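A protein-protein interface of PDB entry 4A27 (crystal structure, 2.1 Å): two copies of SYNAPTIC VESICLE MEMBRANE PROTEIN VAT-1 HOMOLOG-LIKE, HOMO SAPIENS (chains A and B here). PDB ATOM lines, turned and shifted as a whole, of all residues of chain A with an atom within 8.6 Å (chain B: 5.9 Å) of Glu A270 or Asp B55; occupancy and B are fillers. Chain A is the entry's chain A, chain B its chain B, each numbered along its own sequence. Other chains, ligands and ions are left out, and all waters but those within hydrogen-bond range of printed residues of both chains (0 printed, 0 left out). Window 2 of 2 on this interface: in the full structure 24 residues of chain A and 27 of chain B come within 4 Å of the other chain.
No position is printed for both chains.
Of the 12 printed residues of chain B, 6 touch a printed residue of chain A. Hydrophobic or aromatic side chains of chain B that line the printed part of chain A: Phe B278. Of the 11 printed residues of chain A, 7 touch a printed residue of chain B. Hydrophobic or aromatic side chains of chain A within 4 Å of the printed part of chain B: Pro A230, Leu A268 and Tyr A269. Among the printed residues, 15 pairs touch across the chains.
O of Glu A270 sits at hydrogen-bond distance from ND2 of Asn B282, 3.0 Å away. The backbone carbonyl oxygen of Glu A270 lies within hydrogen-bond range of the side-chain amide nitrogen of Gln B287 (3.1 Å). The side-chain amide oxygen (OD1) of Asn A272 is in hydrogen-bond range of the backbone NH (N) of Ser B279. OE1 of Gln B287 sits at hydrogen-bond distance from ND2 of Asn A272, 2.8 Å away. O of Lys A273 sits at hydrogen-bond distance from N of Gly B277. The backbone carbonyl oxygen (O) of Leu A268 sits close to the backbone carbonyl oxygen (O) of Gly B277 (3.4 Å). The side-chain carboxylate of Glu A270 sits close to the side-chain carboxylate of Asp B55 (2.8 Å).
Of chain B, only Asp B55 (2.8 Å), Asn B282 (3.0 Å) and Gln B287 (3.1 Å) come within 4 Å of Glu A270. Printed residues of chain B within 4 Å of Glu A271: Gln B287. Asn B53 touches none of the printed residues of chain A. Of chain A, only Glu A270 comes within 4 Å of Asp B55. Pro B57 touches none of the printed residues of chain A. Printed residues of chain A within 4 Å of Asn B282: Glu A270 and Asn A272. The nearest residue of chain A that does not touch Asp B55 is Tyr A269 (6.7 Å). The nearest printed residue of chain B that does not touch Asn A272 is Lys B286 (7.3 Å).
The backbone carbonyl oxygen (O) of Leu A268 is in hydrogen-bond range of the backbone NH (N) of Lys A273 (3.1 Å). The side-chain amino group of Lys A273 is in salt-bridge range of the side-chain carboxylate of Glu A271, at 3.7 Å. OD2 of Asp B55 is in salt-bridge range of NZ of Lys B286 (3.2 Å). The side-chain hydroxyl (OG) of Ser B279 sits at hydrogen-bond distance from the backbone NH (N) of Asn B282, at 3.2 Å. The side-chain amino group of Lys B286 sits close to the side-chain amide oxygen of Asn B282 (3.5 Å). O of Asn B282 sits at hydrogen-bond distance from N of Gln B287.
Among the printed residues, merely in contact across the chains: Pro A230 with Gln B287, Tyr A269 with Gly B277, Tyr A269 with Phe B278, Tyr A269 with Ser B279, Glu A271 with Gln B287, Asn A272 with Gly B277, Asn A272 with Phe B278 and Asn A272 with Asn B282.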
ATOM      1  N   PRO A 230      17.525  22.316 -28.981  1.00  0.00           N
ATOM      2  CA  PRO A 230      17.324  21.284 -27.989  1.00  0.00           C
ATOM      3  C   PRO A 230      17.303  21.871 -26.577  1.00  0.00           C
ATOM      4  O   PRO A 230      18.084  22.782 -26.273  1.00  0.00           O
ATOM      5  CB  PRO A 230      18.567  20.360 -28.158  1.00  0.00           C
ATOM      6  CG  PRO A 230      19.074  20.641 -29.524  1.00  0.00           C
ATOM      7  CD  PRO A 230      18.721  22.073 -29.812  1.00  0.00           C
ATOM      8  N   ASN A 264       2.034  16.154 -29.953  1.00  0.00           N
ATOM      9  CA  ASN A 264       2.362  14.745 -29.706  1.00  0.00           C
ATOM     10  C   ASN A 264       3.507  14.601 -28.698  1.00  0.00           C
ATOM     11  O   ASN A 264       4.648  14.859 -29.055  1.00  0.00           O
ATOM     12  CB  ASN A 264       2.756  14.056 -31.016  1.00  0.00           C
ATOM     13  N   PRO A 265       3.212  14.193 -27.442  1.00  0.00           N
ATOM     14  CA  PRO A 265       4.223  14.057 -26.364  1.00  0.00           C
ATOM     15  C   PRO A 265       5.494  13.239 -26.692  1.00  0.00           C
ATOM     16  O   PRO A 265       6.556  13.492 -26.102  1.00  0.00           O
ATOM     17  CB  PRO A 265       3.440  13.377 -25.237  1.00  0.00           C
ATOM     18  CG  PRO A 265       2.028  13.792 -25.448  1.00  0.00           C
ATOM     19  CD  PRO A 265       1.841  14.000 -26.929  1.00  0.00           C
ATOM     20  N   ILE A 266       5.393  12.278 -27.606  1.00  0.00           N
ATOM     21  CA  ILE A 266       6.566  11.536 -28.065  1.00  0.00           C
ATOM     22  C   ILE A 266       7.491  12.451 -28.887  1.00  0.00           C
ATOM     23  O   ILE A 266       8.704  12.275 -28.858  1.00  0.00           O
ATOM     24  CB  ILE A 266       6.170  10.279 -28.885  1.00  0.00           C
ATOM     25  N   LYS A 267       6.924  13.427 -29.604  1.00  0.00           N
ATOM     26  CA  LYS A 267       7.723  14.490 -30.272  1.00  0.00           C
ATOM     27  C   LYS A 267       8.568  15.315 -29.280  1.00  0.00           C
ATOM     28  O   LYS A 267       9.705  15.676 -29.571  1.00  0.00           O
ATOM     29  CB  LYS A 267       6.812  15.442 -31.062  1.00  0.00           C
ATOM     30  CG  LYS A 267       7.544  16.478 -31.910  1.00  0.00           C
ATOM     31  N   LEU A 268       8.007  15.608 -28.113  1.00  0.00           N
ATOM     32  CA  LEU A 268       8.734  16.342 -27.086  1.00  0.00           C
ATOM     33  C   LEU A 268       9.918  15.504 -26.587  1.00  0.00           C
ATOM     34  O   LEU A 268      11.046  16.013 -26.482  1.00  0.00           O
ATOM     35  CB  LEU A 268       7.792  16.718 -25.932  1.00  0.00           C
ATOM     36  CG  LEU A 268       6.595  17.639 -26.241  1.00  0.00           C
ATOM     37  CD1 LEU A 268       5.855  18.051 -24.981  1.00  0.00           C
ATOM     38  CD2 LEU A 268       7.026  18.882 -26.985  1.00  0.00           C
ATOM     39  N   TYR A 269       9.644  14.232 -26.285  1.00  0.00           N
ATOM     40  CA  TYR A 269      10.669  13.237 -25.895  1.00  0.00           C
ATOM     41  C   TYR A 269      11.787  13.140 -26.938  1.00  0.00           C
ATOM     42  O   TYR A 269      12.975  13.293 -26.626  1.00  0.00           O
ATOM     43  CB  TYR A 269      10.014  11.856 -25.676  1.00  0.00           C
ATOM     44  CG  TYR A 269      10.968  10.671 -25.533  1.00  0.00           C
ATOM     45  CD1 TYR A 269      11.778  10.542 -24.405  1.00  0.00           C
ATOM     46  CD2 TYR A 269      11.060   9.690 -26.517  1.00  0.00           C
ATOM     47  CE1 TYR A 269      12.672   9.476 -24.260  1.00  0.00           C
ATOM     48  CE2 TYR A 269      11.940   8.609 -26.378  1.00  0.00           C
ATOM     49  CZ  TYR A 269      12.740   8.509 -25.235  1.00  0.00           C
ATOM     50  OH  TYR A 269      13.630   7.476 -25.058  1.00  0.00           O
ATOM     51  N   GLU A 270      11.385  12.937 -28.179  1.00  0.00           N
ATOM     52  CA  GLU A 270      12.330  12.717 -29.272  1.00  0.00           C
ATOM     53  C   GLU A 270      13.118  13.980 -29.562  1.00  0.00           C
ATOM     54  O   GLU A 270      14.327  13.922 -29.805  1.00  0.00           O
ATOM     55  CB  GLU A 270      11.593  12.250 -30.535  1.00  0.00           C
ATOM     56  CG  GLU A 270      10.954  10.850 -30.423  1.00  0.00           C
ATOM     57  CD  GLU A 270      11.853   9.710 -30.908  1.00  0.00           C
ATOM     58  OE1 GLU A 270      12.821   9.966 -31.663  1.00  0.00           O
ATOM     59  OE2 GLU A 270      11.579   8.546 -30.536  1.00  0.00           O
ATOM     60  N   GLU A 271      12.443  15.126 -29.520  1.00  0.00           N
ATOM     61  CA  GLU A 271      13.108  16.374 -29.856  1.00  0.00           C
ATOM     62  C   GLU A 271      13.669  17.122 -28.659  1.00  0.00           C
ATOM     63  O   GLU A 271      14.309  18.162 -28.824  1.00  0.00           O
ATOM     64  CB  GLU A 271      12.176  17.253 -30.668  1.00  0.00           C
ATOM     65  CG  GLU A 271      11.751  16.536 -31.947  1.00  0.00           C
ATOM     66  CD  GLU A 271      10.780  17.293 -32.797  1.00  0.00           C
ATOM     67  OE1 GLU A 271      10.616  18.511 -32.579  1.00  0.00           O
ATOM     68  OE2 GLU A 271      10.189  16.657 -33.696  1.00  0.00           O
ATOM     69  N   ASN A 272      13.430  16.611 -27.453  1.00  0.00           N
ATOM     70  CA  ASN A 272      13.914  17.268 -26.254  1.00  0.00           C
ATOM     71  C   ASN A 272      13.459  18.705 -26.077  1.00  0.00           C
ATOM     72  O   ASN A 272      14.277  19.631 -25.822  1.00  0.00           O
ATOM     73  CB  ASN A 272      15.441  17.216 -26.203  1.00  0.00           C
ATOM     74  CG  ASN A 272      15.928  15.850 -25.892  1.00  0.00           C
ATOM     75  OD1 ASN A 272      15.610  15.299 -24.833  1.00  0.00           O
ATOM     76  ND2 ASN A 272      16.719  15.289 -26.803  1.00  0.00           N
ATOM     77  N   LYS A 273      12.156  18.885 -26.173  1.00  0.00           N
ATOM     78  CA  LYS A 273      11.578  20.215 -26.055  1.00  0.00           C
ATOM     79  C   LYS A 273      10.506  20.332 -24.970  1.00  0.00           C
ATOM     80  O   LYS A 273       9.999  19.330 -24.473  1.00  0.00           O
ATOM     81  CB  LYS A 273      11.060  20.634 -27.414  1.00  0.00           C
ATOM     82  CG  LYS A 273      12.190  21.118 -28.319  1.00  0.00           C
ATOM     83  CD  LYS A 273      11.829  21.018 -29.798  1.00  0.00           C
ATOM     84  CE  LYS A 273      13.075  21.258 -30.693  1.00  0.00           C
ATOM     85  NZ  LYS A 273      12.725  21.516 -32.148  1.00  0.00           N
ATOM     86  N   ASN B  53      11.948  -2.250 -30.303  1.00  0.00           N
ATOM     87  CA  ASN B  53      11.098  -1.101 -29.932  1.00  0.00           C
ATOM     88  C   ASN B  53      11.917   0.179 -29.872  1.00  0.00           C
ATOM     89  O   ASN B  53      12.124   0.744 -28.800  1.00  0.00           O
ATOM     90  CB  ASN B  53      10.453  -1.353 -28.568  1.00  0.00           C
ATOM     91  CG  ASN B  53       9.567  -2.597 -28.568  1.00  0.00           C
ATOM     92  OD1 ASN B  53       8.876  -2.880 -29.550  1.00  0.00           O
ATOM     93  ND2 ASN B  53       9.606  -3.359 -27.472  1.00  0.00           N
ATOM     94  N   ILE B  54      12.396   0.615 -31.027  1.00  0.00           N
ATOM     95  CA  ILE B  54      13.358   1.687 -31.110  1.00  0.00           C
ATOM     96  C   ILE B  54      12.997   2.589 -32.297  1.00  0.00           C
ATOM     97  O   ILE B  54      12.515   2.124 -33.337  1.00  0.00           O
ATOM     98  CB  ILE B  54      14.796   1.117 -31.250  1.00  0.00           C
ATOM     99  N   ASP B  55      13.231   3.884 -32.131  1.00  0.00           N
ATOM    100  CA  ASP B  55      12.942   4.848 -33.182  1.00  0.00           C
ATOM    101  C   ASP B  55      14.037   4.753 -34.229  1.00  0.00           C
ATOM    102  O   ASP B  55      15.210   4.986 -33.924  1.00  0.00           O
ATOM    103  CB  ASP B  55      12.884   6.269 -32.618  1.00  0.00           C
ATOM    104  CG  ASP B  55      12.769   7.326 -33.705  1.00  0.00           C
ATOM    105  OD1 ASP B  55      11.853   7.205 -34.555  1.00  0.00           O
ATOM    106  OD2 ASP B  55      13.599   8.268 -33.712  1.00  0.00           O
ATOM    107  N   ASN B  56      13.644   4.409 -35.454  1.00  0.00           N
ATOM    108  CA  ASN B  56      14.580   4.218 -36.556  1.00  0.00           C
ATOM    109  C   ASN B  56      15.539   3.072 -36.201  1.00  0.00           C
ATOM    110  O   ASN B  56      16.764   3.263 -36.126  1.00  0.00           O
ATOM    111  CB  ASN B  56      15.331   5.529 -36.860  1.00  0.00           C
ATOM    112  CG  ASN B  56      15.996   5.531 -38.237  1.00  0.00           C
ATOM    113  OD1 ASN B  56      15.422   5.071 -39.218  1.00  0.00           O
ATOM    114  ND2 ASN B  56      17.211   6.066 -38.308  1.00  0.00           N
ATOM    115  N   PRO B  57      14.981   1.868 -35.964  1.00  0.00           N
ATOM    116  CA  PRO B  57      15.811   0.782 -35.453  1.00  0.00           C
ATOM    117  C   PRO B  57      17.011   0.533 -36.361  1.00  0.00           C
ATOM    118  O   PRO B  57      16.863   0.548 -37.585  1.00  0.00           O
ATOM    119  CB  PRO B  57      14.861  -0.422 -35.444  1.00  0.00           C
ATOM    120  CG  PRO B  57      13.796  -0.089 -36.407  1.00  0.00           C
ATOM    121  CD  PRO B  57      13.645   1.395 -36.370  1.00  0.00           C
ATOM    122  N   PRO B  58      18.201   0.330 -35.771  1.00  0.00           N
ATOM    123  CA  PRO B  58      19.386   0.084 -36.586  1.00  0.00           C
ATOM    124  C   PRO B  58      19.382  -1.330 -37.148  1.00  0.00           C
ATOM    125  O   PRO B  58      18.589  -2.165 -36.710  1.00  0.00           O
ATOM    126  CB  PRO B  58      20.530   0.260 -35.599  1.00  0.00           C
ATOM    127  CG  PRO B  58      19.947  -0.136 -34.300  1.00  0.00           C
ATOM    128  CD  PRO B  58      18.492   0.210 -34.330  1.00  0.00           C
ATOM    129  N   GLY B 277       9.782  16.639 -22.676  1.00  0.00           N
ATOM    130  CA  GLY B 277      10.212  15.284 -22.984  1.00  0.00           C
ATOM    131  C   GLY B 277      11.704  15.260 -23.010  1.00  0.00           C
ATOM    132  O   GLY B 277      12.315  16.273 -23.311  1.00  0.00           O
ATOM    133  N   PHE B 278      12.293  14.127 -22.625  1.00  0.00           N
ATOM    134  CA  PHE B 278      13.723  14.041 -22.532  1.00  0.00           C
ATOM    135  C   PHE B 278      14.294  12.674 -22.962  1.00  0.00           C
ATOM    136  O   PHE B 278      13.897  11.655 -22.435  1.00  0.00           O
ATOM    137  CB  PHE B 278      14.197  14.377 -21.132  1.00  0.00           C
ATOM    138  CG  PHE B 278      15.699  14.401 -21.016  1.00  0.00           C
ATOM    139  CD1 PHE B 278      16.444  15.367 -21.683  1.00  0.00           C
ATOM    140  CD2 PHE B 278      16.374  13.432 -20.294  1.00  0.00           C
ATOM    141  CE1 PHE B 278      17.843  15.380 -21.595  1.00  0.00           C
ATOM    142  CE2 PHE B 278      17.779  13.435 -20.220  1.00  0.00           C
ATOM    143  CZ  PHE B 278      18.514  14.400 -20.890  1.00  0.00           C
ATOM    144  N   SER B 279      15.238  12.711 -23.899  1.00  0.00           N
ATOM    145  CA  SER B 279      15.930  11.521 -24.425  1.00  0.00           C
ATOM    146  C   SER B 279      17.402  11.859 -24.452  1.00  0.00           C
ATOM    147  O   SER B 279      17.827  12.670 -25.306  1.00  0.00           O
ATOM    148  CB  SER B 279      15.484  11.259 -25.876  1.00  0.00           C
ATOM    149  OG  SER B 279      16.446  10.437 -26.527  1.00  0.00           O
ATOM    150  N   ASN B 282      19.337  10.901 -27.822  1.00  0.00           N
ATOM    151  CA  ASN B 282      19.105  11.845 -28.916  1.00  0.00           C
ATOM    152  C   ASN B 282      19.832  13.133 -28.744  1.00  0.00           C
ATOM    153  O   ASN B 282      20.323  13.709 -29.731  1.00  0.00           O
ATOM    154  CB  ASN B 282      17.624  12.154 -29.092  1.00  0.00           C
ATOM    155  CG  ASN B 282      16.864  11.015 -29.701  1.00  0.00           C
ATOM    156  OD1 ASN B 282      17.427   9.964 -30.036  1.00  0.00           O
ATOM    157  ND2 ASN B 282      15.576  11.195 -29.827  1.00  0.00           N
ATOM    158  N   LYS B 286      22.130  12.772 -31.891  1.00  0.00           N
ATOM    159  CA  LYS B 286      21.359  13.397 -32.982  1.00  0.00           C
ATOM    160  C   LYS B 286      21.357  14.923 -32.934  1.00  0.00           C
ATOM    161  O   LYS B 286      21.337  15.558 -33.979  1.00  0.00           O
ATOM    162  CB  LYS B 286      19.903  12.955 -32.956  1.00  0.00           C
ATOM    163  CG  LYS B 286      19.726  11.495 -33.079  1.00  0.00           C
ATOM    164  CD  LYS B 286      18.267  11.141 -33.268  1.00  0.00           C
ATOM    165  CE  LYS B 286      18.077   9.617 -33.261  1.00  0.00           C
ATOM    166  NZ  LYS B 286      16.627   9.225 -33.313  1.00  0.00           N
ATOM    167  N   GLN B 287      21.379  15.507 -31.731  1.00  0.00           N
ATOM    168  CA  GLN B 287      21.199  16.965 -31.572  1.00  0.00           C
ATOM    169  C   GLN B 287      22.475  17.725 -31.208  1.00  0.00           C
ATOM    170  O   GLN B 287      22.467  18.926 -31.119  1.00  0.00           O
ATOM    171  CB  GLN B 287      20.119  17.226 -30.522  1.00  0.00           C
ATOM    172  CG  GLN B 287      18.729  16.817 -30.999  1.00  0.00           C
ATOM    173  CD  GLN B 287      17.789  16.512 -29.855  1.00  0.00           C
ATOM    174  OE1 GLN B 287      18.073  16.817 -28.691  1.00  0.00           O
ATOM    175  NE2 GLN B 287      16.669  15.897 -30.174  1.00  0.00           N
